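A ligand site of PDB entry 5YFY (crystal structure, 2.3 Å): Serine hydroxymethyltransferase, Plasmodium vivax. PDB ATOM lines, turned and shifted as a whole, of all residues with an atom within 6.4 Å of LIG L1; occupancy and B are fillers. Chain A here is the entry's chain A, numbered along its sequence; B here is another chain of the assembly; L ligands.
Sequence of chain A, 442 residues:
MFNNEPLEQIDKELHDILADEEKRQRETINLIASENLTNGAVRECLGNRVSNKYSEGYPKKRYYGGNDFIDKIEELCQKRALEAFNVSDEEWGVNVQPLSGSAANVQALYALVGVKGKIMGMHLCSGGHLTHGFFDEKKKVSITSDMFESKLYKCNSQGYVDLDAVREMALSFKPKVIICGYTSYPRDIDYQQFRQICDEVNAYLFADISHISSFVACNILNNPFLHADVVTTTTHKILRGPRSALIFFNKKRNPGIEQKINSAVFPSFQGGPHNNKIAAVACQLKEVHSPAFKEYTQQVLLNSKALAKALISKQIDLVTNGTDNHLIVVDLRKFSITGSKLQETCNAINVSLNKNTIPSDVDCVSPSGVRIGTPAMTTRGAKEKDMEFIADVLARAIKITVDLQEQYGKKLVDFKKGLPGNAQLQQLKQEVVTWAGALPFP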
ATOM      1  N   HIS A 123      15.291 -17.017  25.532  1.00  0.00           N
ATOM      2  CA  HIS A 123      15.646 -15.823  26.293  1.00  0.00           C
ATOM      3  C   HIS A 123      16.113 -14.716  25.329  1.00  0.00           C
ATOM      4  O   HIS A 123      16.768 -14.987  24.297  1.00  0.00           O
ATOM      5  CB  HIS A 123      16.741 -16.178  27.298  1.00  0.00           C
ATOM      6  CG  HIS A 123      16.838 -15.263  28.471  1.00  0.00           C
ATOM      7  ND1 HIS A 123      17.442 -14.030  28.398  1.00  0.00           N
ATOM      8  CD2 HIS A 123      16.455 -15.406  29.758  1.00  0.00           C
ATOM      9  CE1 HIS A 123      17.414 -13.443  29.581  1.00  0.00           C
ATOM     10  NE2 HIS A 123      16.807 -14.253  30.427  1.00  0.00           N
ATOM     11  N   LEU A 124      15.770 -13.482  25.640  1.00  0.00           N
ATOM     12  CA  LEU A 124      16.177 -12.318  24.842  1.00  0.00           C
ATOM     13  C   LEU A 124      17.684 -12.281  24.630  1.00  0.00           C
ATOM     14  O   LEU A 124      18.159 -12.128  23.498  1.00  0.00           O
ATOM     15  CB  LEU A 124      15.713 -11.026  25.524  1.00  0.00           C
ATOM     16  CG  LEU A 124      15.958  -9.661  24.866  1.00  0.00           C
ATOM     17  CD1 LEU A 124      14.950  -9.344  23.794  1.00  0.00           C
ATOM     18  CD2 LEU A 124      15.894  -8.571  25.926  1.00  0.00           C
ATOM     19  N   CYS A 125      18.429 -12.381  25.737  1.00  0.00           N
ATOM     20  CA  CYS A 125      19.898 -12.542  25.767  1.00  0.00           C
ATOM     21  C   CYS A 125      20.505 -13.685  24.925  1.00  0.00           C
ATOM     22  O   CYS A 125      21.683 -13.628  24.612  1.00  0.00           O
ATOM     23  CB  CYS A 125      20.400 -12.705  27.226  1.00  0.00           C
ATOM     24  SG  CYS A 125      19.982 -11.370  28.398  1.00  0.00           S
ATOM     25  N   SER A 126      19.722 -14.706  24.587  1.00  0.00           N
ATOM     26  CA  SER A 126      20.185 -15.773  23.717  1.00  0.00           C
ATOM     27  C   SER A 126      19.686 -15.633  22.287  1.00  0.00           C
ATOM     28  O   SER A 126      19.937 -16.517  21.457  1.00  0.00           O
ATOM     29  CB  SER A 126      19.733 -17.140  24.266  1.00  0.00           C
ATOM     30  OG  SER A 126      19.838 -17.200  25.681  1.00  0.00           O
ATOM     31  N   GLY A 127      18.962 -14.551  21.980  1.00  0.00           N
ATOM     32  CA  GLY A 127      18.441 -14.326  20.626  1.00  0.00           C
ATOM     33  C   GLY A 127      16.936 -14.366  20.457  1.00  0.00           C
ATOM     34  O   GLY A 127      16.458 -14.211  19.348  1.00  0.00           O
ATOM     35  N   GLY A 128      16.173 -14.563  21.533  1.00  0.00           N
ATOM     36  CA  GLY A 128      14.717 -14.485  21.457  1.00  0.00           C
ATOM     37  C   GLY A 128      14.221 -13.049  21.315  1.00  0.00           C
ATOM     38  O   GLY A 128      15.006 -12.113  21.468  1.00  0.00           O
ATOM     39  N   HIS A 129      12.941 -12.901  20.973  1.00  0.00           N
ATOM     40  CA  HIS A 129      12.292 -11.587  20.993  1.00  0.00           C
ATOM     41  C   HIS A 129      11.680 -11.277  22.346  1.00  0.00           C
ATOM     42  O   HIS A 129      11.464 -12.165  23.167  1.00  0.00           O
ATOM     43  CB  HIS A 129      11.229 -11.463  19.896  1.00  0.00           C
ATOM     44  CG  HIS A 129      10.811 -10.049  19.618  1.00  0.00           C
ATOM     45  ND1 HIS A 129       9.542  -9.591  19.871  1.00  0.00           N
ATOM     46  CD2 HIS A 129      11.514  -8.973  19.180  1.00  0.00           C
ATOM     47  CE1 HIS A 129       9.465  -8.297  19.589  1.00  0.00           C
ATOM     48  NE2 HIS A 129      10.649  -7.911  19.151  1.00  0.00           N
ATOM     49  N   LEU A 130      11.420  -9.990  22.585  1.00  0.00           N
ATOM     50  CA  LEU A 130      10.716  -9.514  23.781  1.00  0.00           C
ATOM     51  C   LEU A 130       9.374 -10.207  23.972  1.00  0.00           C
ATOM     52  O   LEU A 130       9.067 -10.687  25.058  1.00  0.00           O
ATOM     53  CB  LEU A 130      10.493  -8.017  23.687  1.00  0.00           C
ATOM     54  CG  LEU A 130      11.773  -7.180  23.697  1.00  0.00           C
ATOM     55  CD1 LEU A 130      11.533  -5.784  23.138  1.00  0.00           C
ATOM     56  CD2 LEU A 130      12.326  -7.124  25.113  1.00  0.00           C
ATOM     57  N   PHE A 134       9.778 -12.485  27.507  1.00  0.00           N
ATOM     58  CA  PHE A 134      10.925 -11.911  28.173  1.00  0.00           C
ATOM     59  C   PHE A 134      10.565 -11.253  29.489  1.00  0.00           C
ATOM     60  O   PHE A 134       9.622 -10.455  29.561  1.00  0.00           O
ATOM     61  CB  PHE A 134      11.689 -10.897  27.328  1.00  0.00           C
ATOM     62  CG  PHE A 134      12.898 -10.385  28.029  1.00  0.00           C
ATOM     63  CD1 PHE A 134      13.951 -11.253  28.348  1.00  0.00           C
ATOM     64  CD2 PHE A 134      12.963  -9.075  28.481  1.00  0.00           C
ATOM     65  CE1 PHE A 134      15.050 -10.812  29.051  1.00  0.00           C
ATOM     66  CE2 PHE A 134      14.063  -8.635  29.193  1.00  0.00           C
ATOM     67  CZ  PHE A 134      15.113  -9.500  29.463  1.00  0.00           C
ATOM     68  N   ASP A 136      12.846 -10.209  33.535  1.00  0.00           N
ATOM     69  CA  ASP A 136      14.077 -10.148  34.312  1.00  0.00           C
ATOM     70  C   ASP A 136      13.733 -10.314  35.797  1.00  0.00           C
ATOM     71  O   ASP A 136      12.566 -10.213  36.178  1.00  0.00           O
ATOM     72  CB  ASP A 136      14.779  -8.792  34.069  1.00  0.00           C
ATOM     73  CG  ASP A 136      16.306  -8.902  34.119  1.00  0.00           C
ATOM     74  OD1 ASP A 136      16.875  -9.824  33.491  1.00  0.00           O
ATOM     75  OD2 ASP A 136      16.934  -8.038  34.779  1.00  0.00           O
ATOM     76  N   VAL A 141       9.199  -7.567  31.994  1.00  0.00           N
ATOM     77  CA  VAL A 141       9.506  -6.561  30.973  1.00  0.00           C
ATOM     78  C   VAL A 141       8.516  -6.601  29.783  1.00  0.00           C
ATOM     79  O   VAL A 141       7.991  -5.573  29.372  1.00  0.00           O
ATOM     80  CB  VAL A 141      10.988  -6.704  30.493  1.00  0.00           C
ATOM     81  CG1 VAL A 141      11.309  -5.767  29.328  1.00  0.00           C
ATOM     82  CG2 VAL A 141      11.950  -6.454  31.655  1.00  0.00           C
ATOM     83  N   THR A 183      15.123 -13.439  16.954  1.00  0.00           N
ATOM     84  CA  THR A 183      15.510 -12.109  16.477  1.00  0.00           C
ATOM     85  C   THR A 183      16.960 -12.042  16.078  1.00  0.00           C
ATOM     86  O   THR A 183      17.285 -11.376  15.121  1.00  0.00           O
ATOM     87  CB  THR A 183      15.167 -10.934  17.426  1.00  0.00           C
ATOM     88  OG1 THR A 183      16.343 -10.440  18.087  1.00  0.00           O
ATOM     89  CG2 THR A 183      14.148 -11.287  18.388  1.00  0.00           C
ATOM     90  N   SER A 184      17.838 -12.731  16.788  1.00  0.00           N
ATOM     91  CA  SER A 184      19.247 -12.734  16.408  1.00  0.00           C
ATOM     92  C   SER A 184      19.840 -14.104  16.558  1.00  0.00           C
ATOM     93  O   SER A 184      20.696 -14.324  17.382  1.00  0.00           O
ATOM     94  CB  SER A 184      20.032 -11.692  17.208  1.00  0.00           C
ATOM     95  OG  SER A 184      19.858 -11.878  18.593  1.00  0.00           O
ATOM     96  N   HIS A 211      12.321 -12.748  10.867  1.00  0.00           N
ATOM     97  CA  HIS A 211      13.683 -12.539  10.330  1.00  0.00           C
ATOM     98  C   HIS A 211      14.023 -13.376   9.096  1.00  0.00           C
ATOM     99  O   HIS A 211      14.841 -12.959   8.299  1.00  0.00           O
ATOM    100  CB  HIS A 211      14.735 -12.734  11.415  1.00  0.00           C
ATOM    101  CG  HIS A 211      15.093 -11.475  12.119  1.00  0.00           C
ATOM    102  ND1 HIS A 211      16.031 -10.603  11.639  1.00  0.00           N
ATOM    103  CD2 HIS A 211      14.597 -10.916  13.247  1.00  0.00           C
ATOM    104  CE1 HIS A 211      16.140  -9.574  12.456  1.00  0.00           C
ATOM    105  NE2 HIS A 211      15.276  -9.734  13.438  1.00  0.00           N
ATOM    106  N   ASN A 354      23.729  -2.975  15.238  1.00  0.00           N
ATOM    107  CA  ASN A 354      23.321  -2.923  16.617  1.00  0.00           C
ATOM    108  C   ASN A 354      24.140  -3.842  17.488  1.00  0.00           C
ATOM    109  O   ASN A 354      24.591  -4.891  17.060  1.00  0.00           O
ATOM    110  CB  ASN A 354      21.812  -3.177  16.788  1.00  0.00           C
ATOM    111  CG  ASN A 354      21.400  -4.584  16.381  1.00  0.00           C
ATOM    112  OD1 ASN A 354      21.065  -4.832  15.214  1.00  0.00           O
ATOM    113  ND2 ASN A 354      21.474  -5.507  17.314  1.00  0.00           N
ATOM    114  N   LYS A 355      24.345  -3.404  18.722  1.00  0.00           N
ATOM    115  CA  LYS A 355      24.929  -4.242  19.761  1.00  0.00           C
ATOM    116  C   LYS A 355      24.020  -5.430  20.044  1.00  0.00           C
ATOM    117  O   LYS A 355      22.789  -5.353  19.895  1.00  0.00           O
ATOM    118  CB  LYS A 355      25.203  -3.443  21.059  1.00  0.00           C
ATOM    119  CG  LYS A 355      24.053  -2.526  21.469  1.00  0.00           C
ATOM    120  CD  LYS A 355      23.927  -2.308  22.961  1.00  0.00           C
ATOM    121  CE  LYS A 355      22.627  -1.584  23.249  1.00  0.00           C
ATOM    122  NZ  LYS A 355      22.700  -0.835  24.516  1.00  0.00           N
ATOM    123  N   ASN A 356      24.643  -6.534  20.456  1.00  0.00           N
ATOM    124  CA  ASN A 356      23.961  -7.798  20.562  1.00  0.00           C
ATOM    125  C   ASN A 356      24.661  -8.710  21.551  1.00  0.00           C
ATOM    126  O   ASN A 356      25.880  -8.854  21.526  1.00  0.00           O
ATOM    127  CB  ASN A 356      23.878  -8.473  19.169  1.00  0.00           C
ATOM    128  CG  ASN A 356      22.706  -9.445  19.066  1.00  0.00           C
ATOM    129  OD1 ASN A 356      21.646  -9.117  18.519  1.00  0.00           O
ATOM    130  ND2 ASN A 356      22.877 -10.622  19.590  1.00  0.00           N
ATOM    131  N   THR A 357      23.876  -9.352  22.395  1.00  0.00           N
ATOM    132  CA  THR A 357      24.388 -10.353  23.320  1.00  0.00           C
ATOM    133  C   THR A 357      25.056 -11.527  22.593  1.00  0.00           C
ATOM    134  O   THR A 357      24.725 -11.843  21.442  1.00  0.00           O
ATOM    135  CB  THR A 357      23.252 -10.881  24.209  1.00  0.00           C
ATOM    136  OG1 THR A 357      22.143 -11.271  23.379  1.00  0.00           O
ATOM    137  CG2 THR A 357      22.793  -9.797  25.181  1.00  0.00           C
ATOM    138  N   CYS A 364      22.076  -8.398  29.762  1.00  0.00           N
ATOM    139  CA  CYS A 364      21.834  -7.579  28.552  1.00  0.00           C
ATOM    140  C   CYS A 364      22.440  -6.154  28.649  1.00  0.00           C
ATOM    141  O   CYS A 364      22.259  -5.325  27.748  1.00  0.00           O
ATOM    142  CB  CYS A 364      20.327  -7.504  28.249  1.00  0.00           C
ATOM    143  SG  CYS A 364      19.774  -8.684  26.988  1.00  0.00           S
ATOM    144  N   VAL A 365      23.121  -5.885  29.768  1.00  0.00           N
ATOM    145  CA  VAL A 365      23.969  -4.692  29.940  1.00  0.00           C
ATOM    146  C   VAL A 365      25.391  -5.106  29.560  1.00  0.00           C
ATOM    147  O   VAL A 365      25.888  -6.154  30.002  1.00  0.00           O
ATOM    148  CB  VAL A 365      23.941  -4.099  31.375  1.00  0.00           C
ATOM    149  CG1 VAL A 365      22.637  -3.350  31.615  1.00  0.00           C
ATOM    150  CG2 VAL A 365      24.172  -5.142  32.474  1.00  0.00           C
ATOM    151  N   PRO A 367      26.524  -5.979  26.295  1.00  0.00           N
ATOM    152  CA  PRO A 367      26.668  -7.087  25.370  1.00  0.00           C
ATOM    153  C   PRO A 367      28.021  -7.055  24.624  1.00  0.00           C
ATOM    154  O   PRO A 367      28.546  -5.978  24.297  1.00  0.00           O
ATOM    155  CB  PRO A 367      25.510  -6.901  24.390  1.00  0.00           C
ATOM    156  CG  PRO A 367      25.139  -5.474  24.502  1.00  0.00           C
ATOM    157  CD  PRO A 367      25.377  -5.122  25.940  1.00  0.00           C
ATOM    158  N   ARG A 371      25.316  -7.342  15.846  1.00  0.00           N
ATOM    159  CA  ARG A 371      24.592  -8.044  14.849  1.00  0.00           C
ATOM    160  C   ARG A 371      24.611  -7.263  13.542  1.00  0.00           C
ATOM    161  O   ARG A 371      24.363  -6.053  13.516  1.00  0.00           O
ATOM    162  CB  ARG A 371      23.160  -8.252  15.309  1.00  0.00           C
ATOM    163  CG  ARG A 371      22.327  -9.138  14.399  1.00  0.00           C
ATOM    164  CD  ARG A 371      20.906  -9.155  14.889  1.00  0.00           C
ATOM    165  NE  ARG A 371      20.281  -7.868  14.666  1.00  0.00           N
ATOM    166  CZ  ARG A 371      18.992  -7.607  14.821  1.00  0.00           C
ATOM    167  NH1 ARG A 371      18.138  -8.569  15.212  1.00  0.00           N
ATOM    168  NH2 ARG A 371      18.566  -6.386  14.564  1.00  0.00           N
ATOM    169  N   GLU B  56      13.423   1.432  18.095  1.00  0.00           N
ATOM    170  CA  GLU B  56      12.906   0.986  19.395  1.00  0.00           C
ATOM    171  C   GLU B  56      13.440   1.826  20.540  1.00  0.00           C
ATOM    172  O   GLU B  56      14.616   2.160  20.571  1.00  0.00           O
ATOM    173  CB  GLU B  56      13.263  -0.488  19.653  1.00  0.00           C
ATOM    174  CG  GLU B  56      12.509  -1.498  18.783  1.00  0.00           C
ATOM    175  CD  GLU B  56      13.018  -2.919  18.995  1.00  0.00           C
ATOM    176  OE1 GLU B  56      14.087  -3.258  18.447  1.00  0.00           O
ATOM    177  OE2 GLU B  56      12.391  -3.707  19.733  1.00  0.00           O
ATOM    178  N   TYR B  63      17.833   2.401  21.236  1.00  0.00           N
ATOM    179  CA  TYR B  63      18.685   1.214  21.261  1.00  0.00           C
ATOM    180  C   TYR B  63      19.701   1.319  20.146  1.00  0.00           C
ATOM    181  O   TYR B  63      20.872   1.026  20.357  1.00  0.00           O
ATOM    182  CB  TYR B  63      17.844  -0.084  21.213  1.00  0.00           C
ATOM    183  CG  TYR B  63      17.305  -0.346  22.594  1.00  0.00           C
ATOM    184  CD1 TYR B  63      16.265   0.430  23.101  1.00  0.00           C
ATOM    185  CD2 TYR B  63      17.901  -1.273  23.458  1.00  0.00           C
ATOM    186  CE1 TYR B  63      15.795   0.261  24.393  1.00  0.00           C
ATOM    187  CE2 TYR B  63      17.431  -1.443  24.759  1.00  0.00           C
ATOM    188  CZ  TYR B  63      16.375  -0.669  25.217  1.00  0.00           C
ATOM    189  OH  TYR B  63      15.861  -0.786  26.493  1.00  0.00           O
ATOM    190  N   TYR B  64      19.265   1.797  18.981  1.00  0.00           N
ATOM    191  CA  TYR B  64      20.140   1.891  17.814  1.00  0.00           C
ATOM    192  C   TYR B  64      20.611   3.298  17.556  1.00  0.00           C
ATOM    193  O   TYR B  64      20.062   4.258  18.085  1.00  0.00           O
ATOM    194  CB  TYR B  64      19.402   1.420  16.568  1.00  0.00           C
ATOM    195  CG  TYR B  64      18.866   0.026  16.619  1.00  0.00           C
ATOM    196  CD1 TYR B  64      19.169  -0.850  17.672  1.00  0.00           C
ATOM    197  CD2 TYR B  64      18.076  -0.448  15.577  1.00  0.00           C
ATOM    198  CE1 TYR B  64      18.666  -2.138  17.676  1.00  0.00           C
ATOM    199  CE2 TYR B  64      17.573  -1.735  15.571  1.00  0.00           C
ATOM    200  CZ  TYR B  64      17.860  -2.571  16.607  1.00  0.00           C
ATOM    201  OH  TYR B  64      17.332  -3.835  16.574  1.00  0.00           O
ATOM    202  N   PHE B 266       6.402   0.725  25.199  1.00  0.00           N
ATOM    203  CA  PHE B 266       7.587  -0.078  24.883  1.00  0.00           C
ATOM    204  C   PHE B 266       8.462  -0.229  26.120  1.00  0.00           C
ATOM    205  O   PHE B 266       8.705   0.753  26.797  1.00  0.00           O
ATOM    206  CB  PHE B 266       8.407   0.588  23.787  1.00  0.00           C
ATOM    207  CG  PHE B 266       9.707  -0.114  23.499  1.00  0.00           C
ATOM    208  CD1 PHE B 266       9.720  -1.299  22.768  1.00  0.00           C
ATOM    209  CD2 PHE B 266      10.926   0.388  23.968  1.00  0.00           C
ATOM    210  CE1 PHE B 266      10.882  -1.972  22.510  1.00  0.00           C
ATOM    211  CE2 PHE B 266      12.099  -0.279  23.689  1.00  0.00           C
ATOM    212  CZ  PHE B 266      12.078  -1.470  22.970  1.00  0.00           C
ATOM    213  N   PRO B 267       8.945  -1.433  26.435  1.00  0.00           N
ATOM    214  CA  PRO B 267       8.794  -2.629  25.632  1.00  0.00           C
ATOM    215  C   PRO B 267       7.688  -3.578  26.088  1.00  0.00           C
ATOM    216  O   PRO B 267       7.681  -4.739  25.650  1.00  0.00           O
ATOM    217  CB  PRO B 267      10.154  -3.304  25.814  1.00  0.00           C
ATOM    218  CG  PRO B 267      10.457  -3.026  27.245  1.00  0.00           C
ATOM    219  CD  PRO B 267       9.905  -1.641  27.534  1.00  0.00           C
HETATM  220  C1  LIG L   1      17.126  -9.371  20.964  1.00  0.00           C
HETATM  221  C2  LIG L   1      18.092  -8.428  21.138  1.00  0.00           C
HETATM  222  C3  LIG L   1      17.808  -6.922  20.917  1.00  0.00           C
HETATM  223  C4  LIG L   1      16.341  -6.661  20.761  1.00  0.00           C
HETATM  224  C5  LIG L   1      15.357  -7.716  20.583  1.00  0.00           C
HETATM  225  C6  LIG L   1      15.486  -5.428  20.729  1.00  0.00           C
HETATM  226  C7  LIG L   1      18.486  -6.527  19.575  1.00  0.00           C
HETATM  227  C8  LIG L   1      18.590  -5.009  19.334  1.00  0.00           C
HETATM  228  C9  LIG L   1      19.665  -5.764  22.255  1.00  0.00           C
HETATM  229  C10 LIG L   1      20.142  -5.095  23.374  1.00  0.00           C
HETATM  230  C11 LIG L   1      17.948  -5.194  24.434  1.00  0.00           C
HETATM  231  N1  LIG L   1      17.046  -4.966  25.519  1.00  0.00           N
HETATM  232  C12 LIG L   1      15.662  -4.562  25.174  1.00  0.00           C
HETATM  233  C13 LIG L   1      15.002  -3.842  26.370  1.00  0.00           C
HETATM  234  O1  LIG L   1      14.685  -4.532  29.953  1.00  0.00           O
HETATM  235  C14 LIG L   1      14.619  -3.948  28.843  1.00  0.00           C
HETATM  236  O2  LIG L   1      14.003  -2.854  28.720  1.00  0.00           O
HETATM  237  C15 LIG L   1      15.330  -4.582  27.659  1.00  0.00           C
HETATM  238  C16 LIG L   1      16.816  -4.502  27.921  1.00  0.00           C
HETATM  239  C17 LIG L   1      17.554  -5.316  26.867  1.00  0.00           C
HETATM  240  C18 LIG L   1      19.301  -4.808  24.468  1.00  0.00           C
HETATM  241  F1  LIG L   1      21.432  -4.746  23.380  1.00  0.00           F
HETATM  242  C19 LIG L   1      17.493  -5.883  23.292  1.00  0.00           C
HETATM  243  C20 LIG L   1      18.319  -6.174  22.169  1.00  0.00           C
HETATM  244  C21 LIG L   1      17.897  -7.174  18.303  1.00  0.00           C
HETATM  245  C22 LIG L   1      19.283  -8.702  21.499  1.00  0.00           C
HETATM  246  N2  LIG L   1      20.396  -8.950  21.826  1.00  0.00           N
HETATM  247  N3  LIG L   1      17.336 -10.667  21.139  1.00  0.00           N
HETATM  248  C23 LIG L   1      15.888  -3.978  20.889  1.00  0.00           C
HETATM  249  N4  LIG L   1      14.217  -5.871  20.547  1.00  0.00           N
HETATM  250  N5  LIG L   1      14.095  -7.273  20.455  1.00  0.00           N
HETATM  251  O3  LIG L   1      15.771  -9.010  20.536  1.00  0.00           O
HETATM  252  N1  LG2 L   2       9.369 -11.035  16.129  1.00  0.00           N
HETATM  253  C1  LG2 L   2      10.683 -11.109  15.922  1.00  0.00           C
HETATM  254  C2  LG2 L   2      11.320 -12.481  15.809  1.00  0.00           C
HETATM  255  C3  LG2 L   2      11.495  -9.870  15.788  1.00  0.00           C
HETATM  256  O1  LG2 L   2      12.823  -9.940  15.600  1.00  0.00           O
HETATM  257  C4  LG2 L   2      10.803  -8.572  15.921  1.00  0.00           C
HETATM  258  C5  LG2 L   2      11.566  -7.245  15.773  1.00  0.00           C
HETATM  259  C6  LG2 L   2       9.325  -8.644  16.130  1.00  0.00           C
HETATM  260  C7  LG2 L   2       8.706  -9.893  16.253  1.00  0.00           C
HETATM  261  C8  LG2 L   2       8.427  -7.453  16.349  1.00  0.00           C
HETATM  262  O2  LG2 L   2       8.221  -6.576  15.271  1.00  0.00           O
HETATM  263  P1  LG2 L   2       7.650  -5.096  15.616  1.00  0.00           P
HETATM  264  O3  LG2 L   2       6.705  -5.147  16.759  1.00  0.00           O
HETATM  265  O4  LG2 L   2       8.918  -4.338  15.934  1.00  0.00           O
HETATM  266  O5  LG2 L   2       7.052  -4.848  14.268  1.00  0.00           O
HETATM  267  C9  LG2 L   2      15.019  -6.458  15.319  1.00  0.00           C
HETATM  268  O6  LG2 L   2      15.826  -5.586  14.997  1.00  0.00           O
HETATM  269  O7  LG2 L   2      15.215  -7.660  15.058  1.00  0.00           O
HETATM  270  C10 LG2 L   2      13.754  -6.045  16.032  1.00  0.00           C
HETATM  271  N2  LG2 L   2      12.901  -7.182  16.324  1.00  0.00           N
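O of Gly 128 lies within hydrogen-bond range of N3 of LIG L1 (2.8 Å).
The side-chain hydroxyl of Thr 183 is in hydrogen-bond range of an oxygen (O3) of LIG L1, 2.9 Å away.
O of Leu 124 sits at hydrogen-bond distance from N3 of LIG L1, 2.9 Å away.
The side-chain carboxylate of Glu 56 of chain B is in hydrogen-bond range of a nitrogen (N4) of LIG L1, 2.9 Å away.
The side-chain hydroxyl (OG1) of Thr 357 is in hydrogen-bond range of a nitrogen (N2) of LIG L1 (3.3 Å).
OH of Tyr 64 of chain B sits at hydrogen-bond distance from O6 of LG2 L2 (2.8 Å).
The guanidinium group of Arg 371 lies within salt-bridge range of an oxygen (O6) of LG2 L2 (2.9 Å).
A ring nitrogen (NE2) of His 211 lies within hydrogen-bond range of an oxygen (O7) of LG2 L2, at 2.6 Å.
The backbone carbonyl oxygen (O) of His 123 sits at hydrogen-bond distance from the backbone NH (N) of Gly 128.
The backbone NH (N) of Thr 183 is in hydrogen-bond range of the backbone carbonyl oxygen (O) of Gly 127, 2.8 Å away.
The backbone carbonyl oxygen (O) of Glu 56 of chain B sits at hydrogen-bond distance from the backbone NH (N) of Tyr 63 of chain B (3.3 Å).
OH of Tyr 64 of chain B lies within hydrogen-bond range of NH2 of Arg 371, 3.5 Å away.
OG1 of Thr 357 sits at hydrogen-bond distance from O of Cys 125.
N of Arg 371 is in hydrogen-bond range of O of Asn 354 (2.8 Å).
The side-chain amide oxygen (OD1) of Asn 356 sits at hydrogen-bond distance from the side-chain hydroxyl (OG) of Ser 184, at 3.3 Å.
The backbone carbonyl oxygen of Gly 127 is in hydrogen-bond range of the backbone NH of Ser 184 (3.3 Å).
Gly 127 touches LIG L1.
His 129 touches LIG L1.
CD1 of Leu 130 touches N4 of LIG L1, at 3.7 Å.
Val 141 touches LIG L1.
Ser 184 touches LIG L1 (OG to N3, 3.8 Å).
ND2 of Asn 354 touches C8 of LIG L1, 3.6 Å away.
Lys 355 touches LIG L1.
Asn 356 touches LIG L1 (OD1 to N2, 3.5 Å).
Cys 364 touches LIG L1 (CB to C17, 3.8 Å).
Pro 367 touches LIG L1 (CG to F1, 3.9 Å).
Arg 371 touches LIG L1.
Tyr 63 of chain B touches LIG L1.
OH of Tyr 64 of chain B touches C8 of LIG L1 (3.3 Å).
Pro 267 of chain B touches LIG L1 (CG to O2, 3.8 Å).
Hydrophobic or aromatic side chains within 4 Å of LIG L1: Leu 124, His 129, Leu 130, Val 141, Pro 367, Tyr 63 of chain B, Tyr 64 of chain B and Pro 267 of chain B.
Within 4 Å of LIG L1: Leu 124, Gly 127, Gly 128, His 129, Leu 130, Val 141, Thr 183, Ser 184, Asn 354, Lys 355, Asn 356, Thr 357, Cys 364, Pro 367, Arg 371, Glu 56 of chain B, Tyr 63 of chain B, Tyr 64 of chain B and Pro 267 of chain B.
The nearest printed residue that does not touch LIG L1 is Phe 134 (4.2 Å).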
